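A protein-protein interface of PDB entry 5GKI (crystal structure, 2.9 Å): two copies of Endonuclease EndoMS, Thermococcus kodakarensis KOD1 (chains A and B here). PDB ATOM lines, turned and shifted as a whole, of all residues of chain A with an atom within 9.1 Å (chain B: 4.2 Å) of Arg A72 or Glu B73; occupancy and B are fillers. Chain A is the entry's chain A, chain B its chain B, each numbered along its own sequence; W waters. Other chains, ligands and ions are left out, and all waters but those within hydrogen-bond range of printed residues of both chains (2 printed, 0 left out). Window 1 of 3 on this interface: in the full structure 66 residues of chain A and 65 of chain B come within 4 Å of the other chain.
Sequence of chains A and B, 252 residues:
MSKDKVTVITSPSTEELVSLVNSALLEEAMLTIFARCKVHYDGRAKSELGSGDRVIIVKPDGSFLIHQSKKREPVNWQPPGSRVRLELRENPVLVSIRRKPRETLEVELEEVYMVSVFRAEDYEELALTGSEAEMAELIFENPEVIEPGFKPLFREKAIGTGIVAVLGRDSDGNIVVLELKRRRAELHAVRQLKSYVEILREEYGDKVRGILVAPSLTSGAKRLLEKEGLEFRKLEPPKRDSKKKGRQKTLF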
ATOM      1  N   LYS A  59     -15.862 -19.081   2.650  1.00  0.00           N
ATOM      2  CA  LYS A  59     -16.983 -19.166   1.710  1.00  0.00           C
ATOM      3  C   LYS A  59     -17.202 -20.614   1.298  1.00  0.00           C
ATOM      4  O   LYS A  59     -16.255 -21.402   1.270  1.00  0.00           O
ATOM      5  CB  LYS A  59     -16.744 -18.299   0.469  1.00  0.00           C
ATOM      6  CG  LYS A  59     -16.369 -16.829   0.743  1.00  0.00           C
ATOM      7  CD  LYS A  59     -16.609 -15.974  -0.496  1.00  0.00           C
ATOM      8  CE  LYS A  59     -16.074 -14.573  -0.344  1.00  0.00           C
ATOM      9  NZ  LYS A  59     -16.360 -13.731  -1.544  1.00  0.00           N
ATOM     10  N   ASP A  61     -17.456 -21.965  -1.434  1.00  0.00           N
ATOM     11  CA  ASP A  61     -16.690 -22.399  -2.608  1.00  0.00           C
ATOM     12  C   ASP A  61     -15.227 -22.648  -2.254  1.00  0.00           C
ATOM     13  O   ASP A  61     -14.405 -22.925  -3.125  1.00  0.00           O
ATOM     14  CB  ASP A  61     -16.811 -21.391  -3.767  1.00  0.00           C
ATOM     15  CG  ASP A  61     -15.977 -20.125  -3.572  1.00  0.00           C
ATOM     16  OD1 ASP A  61     -15.470 -19.851  -2.459  1.00  0.00           O
ATOM     17  OD2 ASP A  61     -15.840 -19.382  -4.568  1.00  0.00           O
ATOM     18  N   SER A  63     -13.270 -20.565  -0.473  1.00  0.00           N
ATOM     19  CA  SER A  63     -12.483 -19.356  -0.299  1.00  0.00           C
ATOM     20  C   SER A  63     -12.324 -19.054   1.160  1.00  0.00           C
ATOM     21  O   SER A  63     -13.237 -19.242   1.960  1.00  0.00           O
ATOM     22  CB  SER A  63     -13.114 -18.186  -1.008  1.00  0.00           C
ATOM     23  OG  SER A  63     -13.540 -18.610  -2.283  1.00  0.00           O
ATOM     24  N   PHE A  64     -11.138 -18.591   1.495  1.00  0.00           N
ATOM     25  CA  PHE A  64     -10.747 -18.465   2.868  1.00  0.00           C
ATOM     26  C   PHE A  64     -10.132 -17.094   3.035  1.00  0.00           C
ATOM     27  O   PHE A  64      -9.099 -16.811   2.437  1.00  0.00           O
ATOM     28  CB  PHE A  64      -9.766 -19.573   3.212  1.00  0.00           C
ATOM     29  CG  PHE A  64      -9.596 -19.803   4.666  1.00  0.00           C
ATOM     30  CD1 PHE A  64      -9.198 -18.786   5.500  1.00  0.00           C
ATOM     31  CD2 PHE A  64      -9.800 -21.047   5.197  1.00  0.00           C
ATOM     32  CE1 PHE A  64      -9.029 -19.004   6.830  1.00  0.00           C
ATOM     33  CE2 PHE A  64      -9.637 -21.262   6.528  1.00  0.00           C
ATOM     34  CZ  PHE A  64      -9.248 -20.235   7.348  1.00  0.00           C
ATOM     35  N   LEU A  65     -10.757 -16.237   3.834  1.00  0.00           N
ATOM     36  CA  LEU A  65     -10.244 -14.883   3.991  1.00  0.00           C
ATOM     37  C   LEU A  65      -9.887 -14.602   5.431  1.00  0.00           C
ATOM     38  O   LEU A  65     -10.636 -14.926   6.348  1.00  0.00           O
ATOM     39  CB  LEU A  65     -11.262 -13.857   3.500  1.00  0.00           C
ATOM     40  CG  LEU A  65     -11.846 -14.093   2.109  1.00  0.00           C
ATOM     41  CD1 LEU A  65     -12.890 -13.048   1.783  1.00  0.00           C
ATOM     42  CD2 LEU A  65     -10.757 -14.091   1.069  1.00  0.00           C
ATOM     43  N   ILE A  66      -8.728 -14.001   5.621  1.00  0.00           N
ATOM     44  CA  ILE A  66      -8.323 -13.519   6.924  1.00  0.00           C
ATOM     45  C   ILE A  66      -8.054 -12.033   6.845  1.00  0.00           C
ATOM     46  O   ILE A  66      -7.169 -11.596   6.121  1.00  0.00           O
ATOM     47  CB  ILE A  66      -7.085 -14.228   7.407  1.00  0.00           C
ATOM     48  CG1 ILE A  66      -7.321 -15.734   7.353  1.00  0.00           C
ATOM     49  CG2 ILE A  66      -6.710 -13.738   8.799  1.00  0.00           C
ATOM     50  CD1 ILE A  66      -6.082 -16.529   7.585  1.00  0.00           C
ATOM     51  N   HIS A  67      -8.827 -11.255   7.587  1.00  0.00           N
ATOM     52  CA  HIS A  67      -8.741  -9.809   7.509  1.00  0.00           C
ATOM     53  C   HIS A  67      -8.270  -9.178   8.807  1.00  0.00           C
ATOM     54  O   HIS A  67      -8.806  -9.456   9.865  1.00  0.00           O
ATOM     55  CB  HIS A  67     -10.090  -9.229   7.131  1.00  0.00           C
ATOM     56  CG  HIS A  67     -10.326  -9.159   5.660  1.00  0.00           C
ATOM     57  ND1 HIS A  67      -9.826  -8.143   4.876  1.00  0.00           N
ATOM     58  CD2 HIS A  67     -11.023  -9.967   4.828  1.00  0.00           C
ATOM     59  CE1 HIS A  67     -10.192  -8.333   3.622  1.00  0.00           C
ATOM     60  NE2 HIS A  67     -10.922  -9.435   3.564  1.00  0.00           N
ATOM     61  N   GLN A  68      -7.251  -8.335   8.721  1.00  0.00           N
ATOM     62  CA  GLN A  68      -6.890  -7.500   9.849  1.00  0.00           C
ATOM     63  C   GLN A  68      -7.696  -6.227   9.759  1.00  0.00           C
ATOM     64  O   GLN A  68      -8.512  -6.079   8.848  1.00  0.00           O
ATOM     65  CB  GLN A  68      -5.413  -7.177   9.846  1.00  0.00           C
ATOM     66  CG  GLN A  68      -4.553  -8.336   9.533  1.00  0.00           C
ATOM     67  CD  GLN A  68      -3.108  -7.942   9.481  1.00  0.00           C
ATOM     68  OE1 GLN A  68      -2.626  -7.437   8.458  1.00  0.00           O
ATOM     69  NE2 GLN A  68      -2.397  -8.151  10.593  1.00  0.00           N
ATOM     70  N   SER A  69      -7.419  -5.287  10.661  1.00  0.00           N
ATOM     71  CA  SER A  69      -8.250  -4.102  10.808  1.00  0.00           C
ATOM     72  C   SER A  69      -7.951  -3.052   9.743  1.00  0.00           C
ATOM     73  O   SER A  69      -8.615  -2.015   9.690  1.00  0.00           O
ATOM     74  CB  SER A  69      -8.067  -3.511  12.201  1.00  0.00           C
ATOM     75  OG  SER A  69      -6.696  -3.322  12.486  1.00  0.00           O
ATOM     76  N   LYS A  70      -6.981  -3.341   8.871  1.00  0.00           N
ATOM     77  CA  LYS A  70      -6.583  -2.400   7.822  1.00  0.00           C
ATOM     78  C   LYS A  70      -6.490  -2.973   6.404  1.00  0.00           C
ATOM     79  O   LYS A  70      -6.563  -4.174   6.172  1.00  0.00           O
ATOM     80  CB  LYS A  70      -5.248  -1.762   8.185  1.00  0.00           C
ATOM     81  CG  LYS A  70      -5.377  -0.538   9.078  1.00  0.00           C
ATOM     82  CD  LYS A  70      -4.035  -0.144   9.701  1.00  0.00           C
ATOM     83  CE  LYS A  70      -4.003  -0.474  11.192  1.00  0.00           C
ATOM     84  NZ  LYS A  70      -5.303  -0.132  11.850  1.00  0.00           N
ATOM     85  N   LYS A  71      -6.335  -2.043   5.477  1.00  0.00           N
ATOM     86  CA  LYS A  71      -6.303  -2.192   4.017  1.00  0.00           C
ATOM     87  C   LYS A  71      -7.523  -2.849   3.341  1.00  0.00           C
ATOM     88  O   LYS A  71      -8.532  -3.065   3.994  1.00  0.00           O
ATOM     89  CB  LYS A  71      -5.053  -3.001   3.673  1.00  0.00           C
ATOM     90  CG  LYS A  71      -3.736  -2.335   4.074  1.00  0.00           C
ATOM     91  CD  LYS A  71      -2.528  -3.235   3.774  1.00  0.00           C
ATOM     92  CE  LYS A  71      -2.856  -4.242   2.660  1.00  0.00           C
ATOM     93  NZ  LYS A  71      -1.709  -5.078   2.188  1.00  0.00           N
ATOM     94  N   ARG A  72      -7.399  -3.255   2.073  1.00  0.00           N
ATOM     95  CA  ARG A  72      -8.517  -3.894   1.341  1.00  0.00           C
ATOM     96  C   ARG A  72      -8.294  -5.382   1.189  1.00  0.00           C
ATOM     97  O   ARG A  72      -9.146  -6.140   0.689  1.00  0.00           O
ATOM     98  CB  ARG A  72      -8.712  -3.291  -0.057  1.00  0.00           C
ATOM     99  CG  ARG A  72     -10.106  -3.576  -0.594  1.00  0.00           C
ATOM    100  CD  ARG A  72     -10.224  -3.792  -2.077  1.00  0.00           C
ATOM    101  NE  ARG A  72      -9.617  -5.031  -2.523  1.00  0.00           N
ATOM    102  CZ  ARG A  72      -9.850  -5.598  -3.702  1.00  0.00           C
ATOM    103  NH1 ARG A  72     -10.722  -5.067  -4.537  1.00  0.00           N
ATOM    104  NH2 ARG A  72      -9.233  -6.723  -4.035  1.00  0.00           N
ATOM    105  N   GLU A  73      -7.104  -5.776   1.603  1.00  0.00           N
ATOM    106  CA  GLU A  73      -6.570  -7.065   1.270  1.00  0.00           C
ATOM    107  C   GLU A  73      -6.520  -7.948   2.467  1.00  0.00           C
ATOM    108  O   GLU A  73      -6.093  -7.526   3.533  1.00  0.00           O
ATOM    109  CB  GLU A  73      -5.201  -6.909   0.635  1.00  0.00           C
ATOM    110  CG  GLU A  73      -5.304  -6.246  -0.709  1.00  0.00           C
ATOM    111  CD  GLU A  73      -6.189  -7.037  -1.646  1.00  0.00           C
ATOM    112  OE1 GLU A  73      -6.122  -8.281  -1.576  1.00  0.00           O
ATOM    113  OE2 GLU A  73      -6.940  -6.429  -2.448  1.00  0.00           O
ATOM    114  N   PRO A  74      -7.028  -9.165   2.311  1.00  0.00           N
ATOM    115  CA  PRO A  74      -6.853 -10.154   3.368  1.00  0.00           C
ATOM    116  C   PRO A  74      -5.365 -10.327   3.626  1.00  0.00           C
ATOM    117  O   PRO A  74      -4.587 -10.232   2.681  1.00  0.00           O
ATOM    118  CB  PRO A  74      -7.480 -11.413   2.782  1.00  0.00           C
ATOM    119  CG  PRO A  74      -7.413 -11.208   1.308  1.00  0.00           C
ATOM    120  CD  PRO A  74      -7.500  -9.756   1.052  1.00  0.00           C
ATOM    121  N   VAL A  75      -4.962 -10.517   4.873  1.00  0.00           N
ATOM    122  CA  VAL A  75      -3.551 -10.676   5.131  1.00  0.00           C
ATOM    123  C   VAL A  75      -3.157 -12.058   4.630  1.00  0.00           C
ATOM    124  O   VAL A  75      -2.169 -12.218   3.925  1.00  0.00           O
ATOM    125  CB  VAL A  75      -3.192 -10.490   6.614  1.00  0.00           C
ATOM    126  CG1 VAL A  75      -4.149 -11.267   7.506  1.00  0.00           C
ATOM    127  CG2 VAL A  75      -1.760 -10.910   6.865  1.00  0.00           C
ATOM    128  N   TRP A  77      -4.931 -15.837   2.909  1.00  0.00           N
ATOM    129  CA  TRP A  77      -6.125 -16.299   2.232  1.00  0.00           C
ATOM    130  C   TRP A  77      -5.946 -17.594   1.482  1.00  0.00           C
ATOM    131  O   TRP A  77      -4.857 -18.109   1.360  1.00  0.00           O
ATOM    132  CB  TRP A  77      -6.593 -15.250   1.236  1.00  0.00           C
ATOM    133  CG  TRP A  77      -5.711 -15.231   0.028  1.00  0.00           C
ATOM    134  CD1 TRP A  77      -5.886 -15.924  -1.138  1.00  0.00           C
ATOM    135  CD2 TRP A  77      -4.495 -14.504  -0.121  1.00  0.00           C
ATOM    136  NE1 TRP A  77      -4.865 -15.649  -2.006  1.00  0.00           N
ATOM    137  CE2 TRP A  77      -3.995 -14.778  -1.400  1.00  0.00           C
ATOM    138  CE3 TRP A  77      -3.785 -13.632   0.702  1.00  0.00           C
ATOM    139  CZ2 TRP A  77      -2.821 -14.219  -1.872  1.00  0.00           C
ATOM    140  CZ3 TRP A  77      -2.619 -13.078   0.230  1.00  0.00           C
ATOM    141  CH2 TRP A  77      -2.146 -13.374  -1.038  1.00  0.00           C
ATOM    142  N   GLN A  78      -7.060 -18.060   0.913  1.00  0.00           N
ATOM    143  CA  GLN A  78      -7.097 -19.213   0.016  1.00  0.00           C
ATOM    144  C   GLN A  78      -8.216 -19.075  -1.033  1.00  0.00           C
ATOM    145  O   GLN A  78      -9.386 -18.901  -0.688  1.00  0.00           O
ATOM    146  CB  GLN A  78      -7.278 -20.507   0.812  1.00  0.00           C
ATOM    147  CG  GLN A  78      -6.005 -21.014   1.469  1.00  0.00           C
ATOM    148  CD  GLN A  78      -5.063 -21.674   0.483  1.00  0.00           C
ATOM    149  OE1 GLN A  78      -4.728 -21.101  -0.554  1.00  0.00           O
ATOM    150  NE2 GLN A  78      -4.628 -22.889   0.802  1.00  0.00           N
ATOM    151  N   PRO A  79      -7.840 -19.155  -2.308  1.00  0.00           N
ATOM    152  CA  PRO A  79      -8.761 -19.052  -3.445  1.00  0.00           C
ATOM    153  C   PRO A  79      -9.759 -20.217  -3.448  1.00  0.00           C
ATOM    154  O   PRO A  79      -9.581 -21.156  -2.679  1.00  0.00           O
ATOM    155  CB  PRO A  79      -7.824 -19.096  -4.653  1.00  0.00           C
ATOM    156  CG  PRO A  79      -6.681 -19.894  -4.187  1.00  0.00           C
ATOM    157  CD  PRO A  79      -6.502 -19.601  -2.727  1.00  0.00           C
ATOM    158  N   PRO A  80     -10.812 -20.144  -4.273  1.00  0.00           N
ATOM    159  CA  PRO A  80     -11.777 -21.244  -4.347  1.00  0.00           C
ATOM    160  C   PRO A  80     -11.138 -22.610  -4.588  1.00  0.00           C
ATOM    161  O   PRO A  80     -10.041 -22.709  -5.146  1.00  0.00           O
ATOM    162  CB  PRO A  80     -12.649 -20.848  -5.534  1.00  0.00           C
ATOM    163  CG  PRO A  80     -12.611 -19.376  -5.526  1.00  0.00           C
ATOM    164  CD  PRO A  80     -11.208 -19.023  -5.141  1.00  0.00           C
ATOM    165  N   SER B  63     -11.689   1.184   4.431  1.00  0.00           N
ATOM    166  CA  SER B  63     -11.885   0.154   3.417  1.00  0.00           C
ATOM    167  C   SER B  63     -13.245  -0.451   3.624  1.00  0.00           C
ATOM    168  O   SER B  63     -13.676  -0.646   4.763  1.00  0.00           O
ATOM    169  CB  SER B  63     -10.832  -0.937   3.514  1.00  0.00           C
ATOM    170  OG  SER B  63      -9.642  -0.421   4.074  1.00  0.00           O
ATOM    171  N   LEU B  65     -15.786  -3.591   2.190  1.00  0.00           N
ATOM    172  CA  LEU B  65     -15.872  -4.800   1.367  1.00  0.00           C
ATOM    173  C   LEU B  65     -17.283  -5.332   1.261  1.00  0.00           C
ATOM    174  O   LEU B  65     -18.049  -5.308   2.216  1.00  0.00           O
ATOM    175  CB  LEU B  65     -14.976  -5.902   1.922  1.00  0.00           C
ATOM    176  CG  LEU B  65     -13.611  -5.399   2.340  1.00  0.00           C
ATOM    177  CD1 LEU B  65     -12.847  -6.476   3.043  1.00  0.00           C
ATOM    178  CD2 LEU B  65     -12.875  -4.916   1.124  1.00  0.00           C
ATOM    179  N   HIS B  67     -18.893  -8.947   0.147  1.00  0.00           N
ATOM    180  CA  HIS B  67     -18.652 -10.304  -0.308  1.00  0.00           C
ATOM    181  C   HIS B  67     -19.907 -11.128  -0.568  1.00  0.00           C
ATOM    182  O   HIS B  67     -20.754 -11.289   0.315  1.00  0.00           O
ATOM    183  CB  HIS B  67     -17.785 -11.029   0.709  1.00  0.00           C
ATOM    184  CG  HIS B  67     -16.332 -10.686   0.611  1.00  0.00           C
ATOM    185  ND1 HIS B  67     -15.517 -11.172  -0.394  1.00  0.00           N
ATOM    186  CD2 HIS B  67     -15.538  -9.914   1.390  1.00  0.00           C
ATOM    187  CE1 HIS B  67     -14.297 -10.707  -0.232  1.00  0.00           C
ATOM    188  NE2 HIS B  67     -14.279  -9.943   0.848  1.00  0.00           N
ATOM    189  N   LYS B  71     -16.255 -16.765  -4.833  1.00  0.00           N
ATOM    190  CA  LYS B  71     -14.946 -16.184  -5.120  1.00  0.00           C
ATOM    191  C   LYS B  71     -14.102 -15.728  -3.919  1.00  0.00           C
ATOM    192  O   LYS B  71     -14.422 -16.020  -2.775  1.00  0.00           O
ATOM    193  CB  LYS B  71     -15.141 -14.973  -6.042  1.00  0.00           C
ATOM    194  CG  LYS B  71     -16.061 -15.208  -7.226  1.00  0.00           C
ATOM    195  CD  LYS B  71     -15.617 -16.407  -8.032  1.00  0.00           C
ATOM    196  CE  LYS B  71     -16.145 -16.365  -9.453  1.00  0.00           C
ATOM    197  NZ  LYS B  71     -15.555 -17.494 -10.229  1.00  0.00           N
ATOM    198  N   ARG B  72     -13.141 -14.854  -4.188  1.00  0.00           N
ATOM    199  CA  ARG B  72     -12.145 -14.430  -3.210  1.00  0.00           C
ATOM    200  C   ARG B  72     -12.259 -12.936  -3.118  1.00  0.00           C
ATOM    201  O   ARG B  72     -12.353 -12.352  -2.044  1.00  0.00           O
ATOM    202  CB  ARG B  72     -10.709 -14.811  -3.574  1.00  0.00           C
ATOM    203  CG  ARG B  72      -9.802 -14.630  -2.360  1.00  0.00           C
ATOM    204  CD  ARG B  72      -8.373 -14.312  -2.636  1.00  0.00           C
ATOM    205  NE  ARG B  72      -8.146 -12.977  -3.186  1.00  0.00           N
ATOM    206  CZ  ARG B  72      -7.100 -12.201  -2.885  1.00  0.00           C
ATOM    207  NH1 ARG B  72      -6.192 -12.593  -2.007  1.00  0.00           N
ATOM    208  NH2 ARG B  72      -6.962 -11.019  -3.455  1.00  0.00           N
ATOM    209  N   GLU B  73     -12.122 -12.323  -4.279  1.00  0.00           N
ATOM    210  CA  GLU B  73     -12.466 -10.936  -4.452  1.00  0.00           C
ATOM    211  C   GLU B  73     -13.871 -10.574  -3.960  1.00  0.00           C
ATOM    212  O   GLU B  73     -14.826 -11.328  -4.143  1.00  0.00           O
ATOM    213  CB  GLU B  73     -12.318 -10.582  -5.932  1.00  0.00           C
ATOM    214  CG  GLU B  73     -10.904 -10.681  -6.378  1.00  0.00           C
ATOM    215  CD  GLU B  73      -9.951 -10.201  -5.300  1.00  0.00           C
ATOM    216  OE1 GLU B  73     -10.079  -9.041  -4.834  1.00  0.00           O
ATOM    217  OE2 GLU B  73      -9.085 -11.007  -4.904  1.00  0.00           O
ATOM    218  N   PRO B  74     -13.989  -9.410  -3.320  1.00  0.00           N
ATOM    219  CA  PRO B  74     -15.280  -8.759  -3.068  1.00  0.00           C
ATOM    220  C   PRO B  74     -16.000  -8.396  -4.372  1.00  0.00           C
ATOM    221  O   PRO B  74     -15.328  -8.121  -5.365  1.00  0.00           O
ATOM    222  CB  PRO B  74     -14.882  -7.501  -2.307  1.00  0.00           C
ATOM    223  CG  PRO B  74     -13.448  -7.270  -2.694  1.00  0.00           C
ATOM    224  CD  PRO B  74     -12.867  -8.628  -2.786  1.00  0.00           C
ATOM    225  N   VAL B  75     -17.333  -8.391  -4.380  1.00  0.00           N
ATOM    226  CA  VAL B  75     -18.069  -8.008  -5.594  1.00  0.00           C
ATOM    227  C   VAL B  75     -17.988  -6.506  -5.806  1.00  0.00           C
ATOM    228  O   VAL B  75     -18.012  -6.009  -6.930  1.00  0.00           O
ATOM    229  CB  VAL B  75     -19.559  -8.445  -5.563  1.00  0.00           C
ATOM    230  CG1 VAL B  75     -20.334  -7.668  -4.540  1.00  0.00           C
ATOM    231  CG2 VAL B  75     -20.178  -8.244  -6.908  1.00  0.00           C
ATOM    232  N   TRP B  77     -16.318  -2.833  -3.602  1.00  0.00           N
ATOM    233  CA  TRP B  77     -15.495  -2.446  -2.487  1.00  0.00           C
ATOM    234  C   TRP B  77     -15.211  -0.984  -2.570  1.00  0.00           C
ATOM    235  O   TRP B  77     -15.627  -0.299  -3.498  1.00  0.00           O
ATOM    236  CB  TRP B  77     -14.169  -3.217  -2.483  1.00  0.00           C
ATOM    237  CG  TRP B  77     -13.374  -2.839  -3.671  1.00  0.00           C
ATOM    238  CD1 TRP B  77     -12.424  -1.866  -3.754  1.00  0.00           C
ATOM    239  CD2 TRP B  77     -13.526  -3.366  -4.987  1.00  0.00           C
ATOM    240  NE1 TRP B  77     -11.948  -1.777  -5.036  1.00  0.00           N
ATOM    241  CE2 TRP B  77     -12.611  -2.689  -5.816  1.00  0.00           C
ATOM    242  CE3 TRP B  77     -14.337  -4.362  -5.545  1.00  0.00           C
ATOM    243  CZ2 TRP B  77     -12.481  -2.971  -7.169  1.00  0.00           C
ATOM    244  CZ3 TRP B  77     -14.208  -4.642  -6.884  1.00  0.00           C
ATOM    245  CH2 TRP B  77     -13.277  -3.952  -7.685  1.00  0.00           C
ATOM    246  N   PRO B  80      -8.780   1.687   1.069  1.00  0.00           N
ATOM    247  CA  PRO B  80      -8.608   2.433   2.323  1.00  0.00           C
ATOM    248  C   PRO B  80      -8.679   3.943   2.137  1.00  0.00           C
ATOM    249  O   PRO B  80      -8.372   4.443   1.059  1.00  0.00           O
ATOM    250  CB  PRO B  80      -7.215   2.019   2.790  1.00  0.00           C
ATOM    251  CG  PRO B  80      -6.997   0.675   2.170  1.00  0.00           C
ATOM    252  CD  PRO B  80      -7.711   0.692   0.858  1.00  0.00           C
HETATM  253  O   HOH W   1     -17.638 -11.692  -3.562  1.00  0.00           O
HETATM  254  O   HOH W   2     -11.523  -9.604   0.892  1.00  0.00           O
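The guanidinium group of Arg B72 lies within salt-bridge range of the side-chain carboxylate of Glu A73 (3.4 Å).
The side-chain amino group (NZ) of Lys A59 lies close to the backbone carbonyl oxygen (O) of Lys B71 (3.2 Å).
The side-chain hydroxyl (OG) of Ser A63 lies within hydrogen-bond range of the backbone carbonyl oxygen (O) of Lys B71 (2.8 Å).
OD2 of Asp A61 lies within hydrogen-bond range of N of Lys B71.
A ring nitrogen (ND1) of His B67 sits at hydrogen-bond distance from the side-chain amino group (NZ) of Lys A59 (2.9 Å).
NE1 of Trp A77 lies close to NH1 of Arg B72.
O of Lys A71 is in hydrogen-bond range of OG of Ser B63 (2.9 Å).
OE1 of Glu B73 is in salt-bridge range of NH2 of Arg A72, at 2.6 Å.
The side-chain carboxylate (OE2) of Glu B73 lies within salt-bridge range of the guanidinium group (NH2) of Arg B72, at 2.6 Å.
The side-chain carboxylate (OD1) of Asp A61 is in hydrogen-bond range of the backbone NH (N) of Ser A63 (3.0 Å).
The guanidinium group (NH2) of Arg A72 lies within salt-bridge range of the side-chain carboxylate (OE2) of Glu A73, at 2.8 Å.
Among the printed residues, merely in contact across the chains: His A67 with Leu B65, Arg A72 with Trp B77, Leu A65 with His B67, Lys A71 with Pro B80, Arg A72 with Leu B65, Leu A65 with Arg B72, Pro A74 with Arg B72, Lys A59 with Glu B73, Arg A72 with Pro B80, Arg A72 with Pro B74 and Pro A80 with Lys B71.
Arg A72 touches five residues of chain B.
Glu B73 touches just these residues of chain A: Lys A59 (3.9 Å) and Arg A72 (2.6 Å).
Pro B74 touches just one residue of chain A: Arg A72 (3.96 Å).
Printed residues of chain A within 4 Å of Trp B77: Arg A72.
Printed residues of chain A within 4 Å of Pro B80: Lys A71 (3.5 Å) and Arg A72 (3.95 Å).
The nearest residue of chain A that does not touch Glu B73 is Glu A73 (4.7 Å).
The nearest printed residue of chain A that does not touch Lys B71 is Leu A65 (5.7 Å).
Of the 19 printed residues of chain A, 11 touch a printed residue of chain B.
Of the 10 printed residues of chain B, 9 touch a printed residue of chain A.
Among the printed residues, Asp or Glu carboxylates within 4 Å of a Lys or Arg side-chain nitrogen of the other chain: Arg A72 with Glu B73 (2.6 Å) and Glu A73 with Arg B72 (3.4 Å).
Leu A65 touches Arg B72, and with the chains exchanged Arg A72 touches Leu B65.
Arg A72 touches Pro B74, and with the chains exchanged Pro A74 touches Arg B72.
Arg A72 touches Trp B77, and with the chains exchanged Trp A77 touches Arg B72.
Arg A72 touches Pro B80, but with the chains exchanged Pro A80 does not touch Arg B72 (4.5 Å).
Of the 19 pairs that touch across the chains among the printed residues, 14 have their exchanged pair printed and touching as well.
Water W2 lies within hydrogen-bond range of a ring nitrogen (NE2) of His A67 (2.7 Å) and a ring nitrogen (NE2) of His B67 (2.8 Å).
Water W1 lies within hydrogen-bond range of the backbone carbonyl oxygen (O) of Glu B73 (2.9 Å), the side-chain amino group (NZ) of Lys A59 (3.1 Å) and the backbone NH (N) of Val B75 (3.4 Å).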
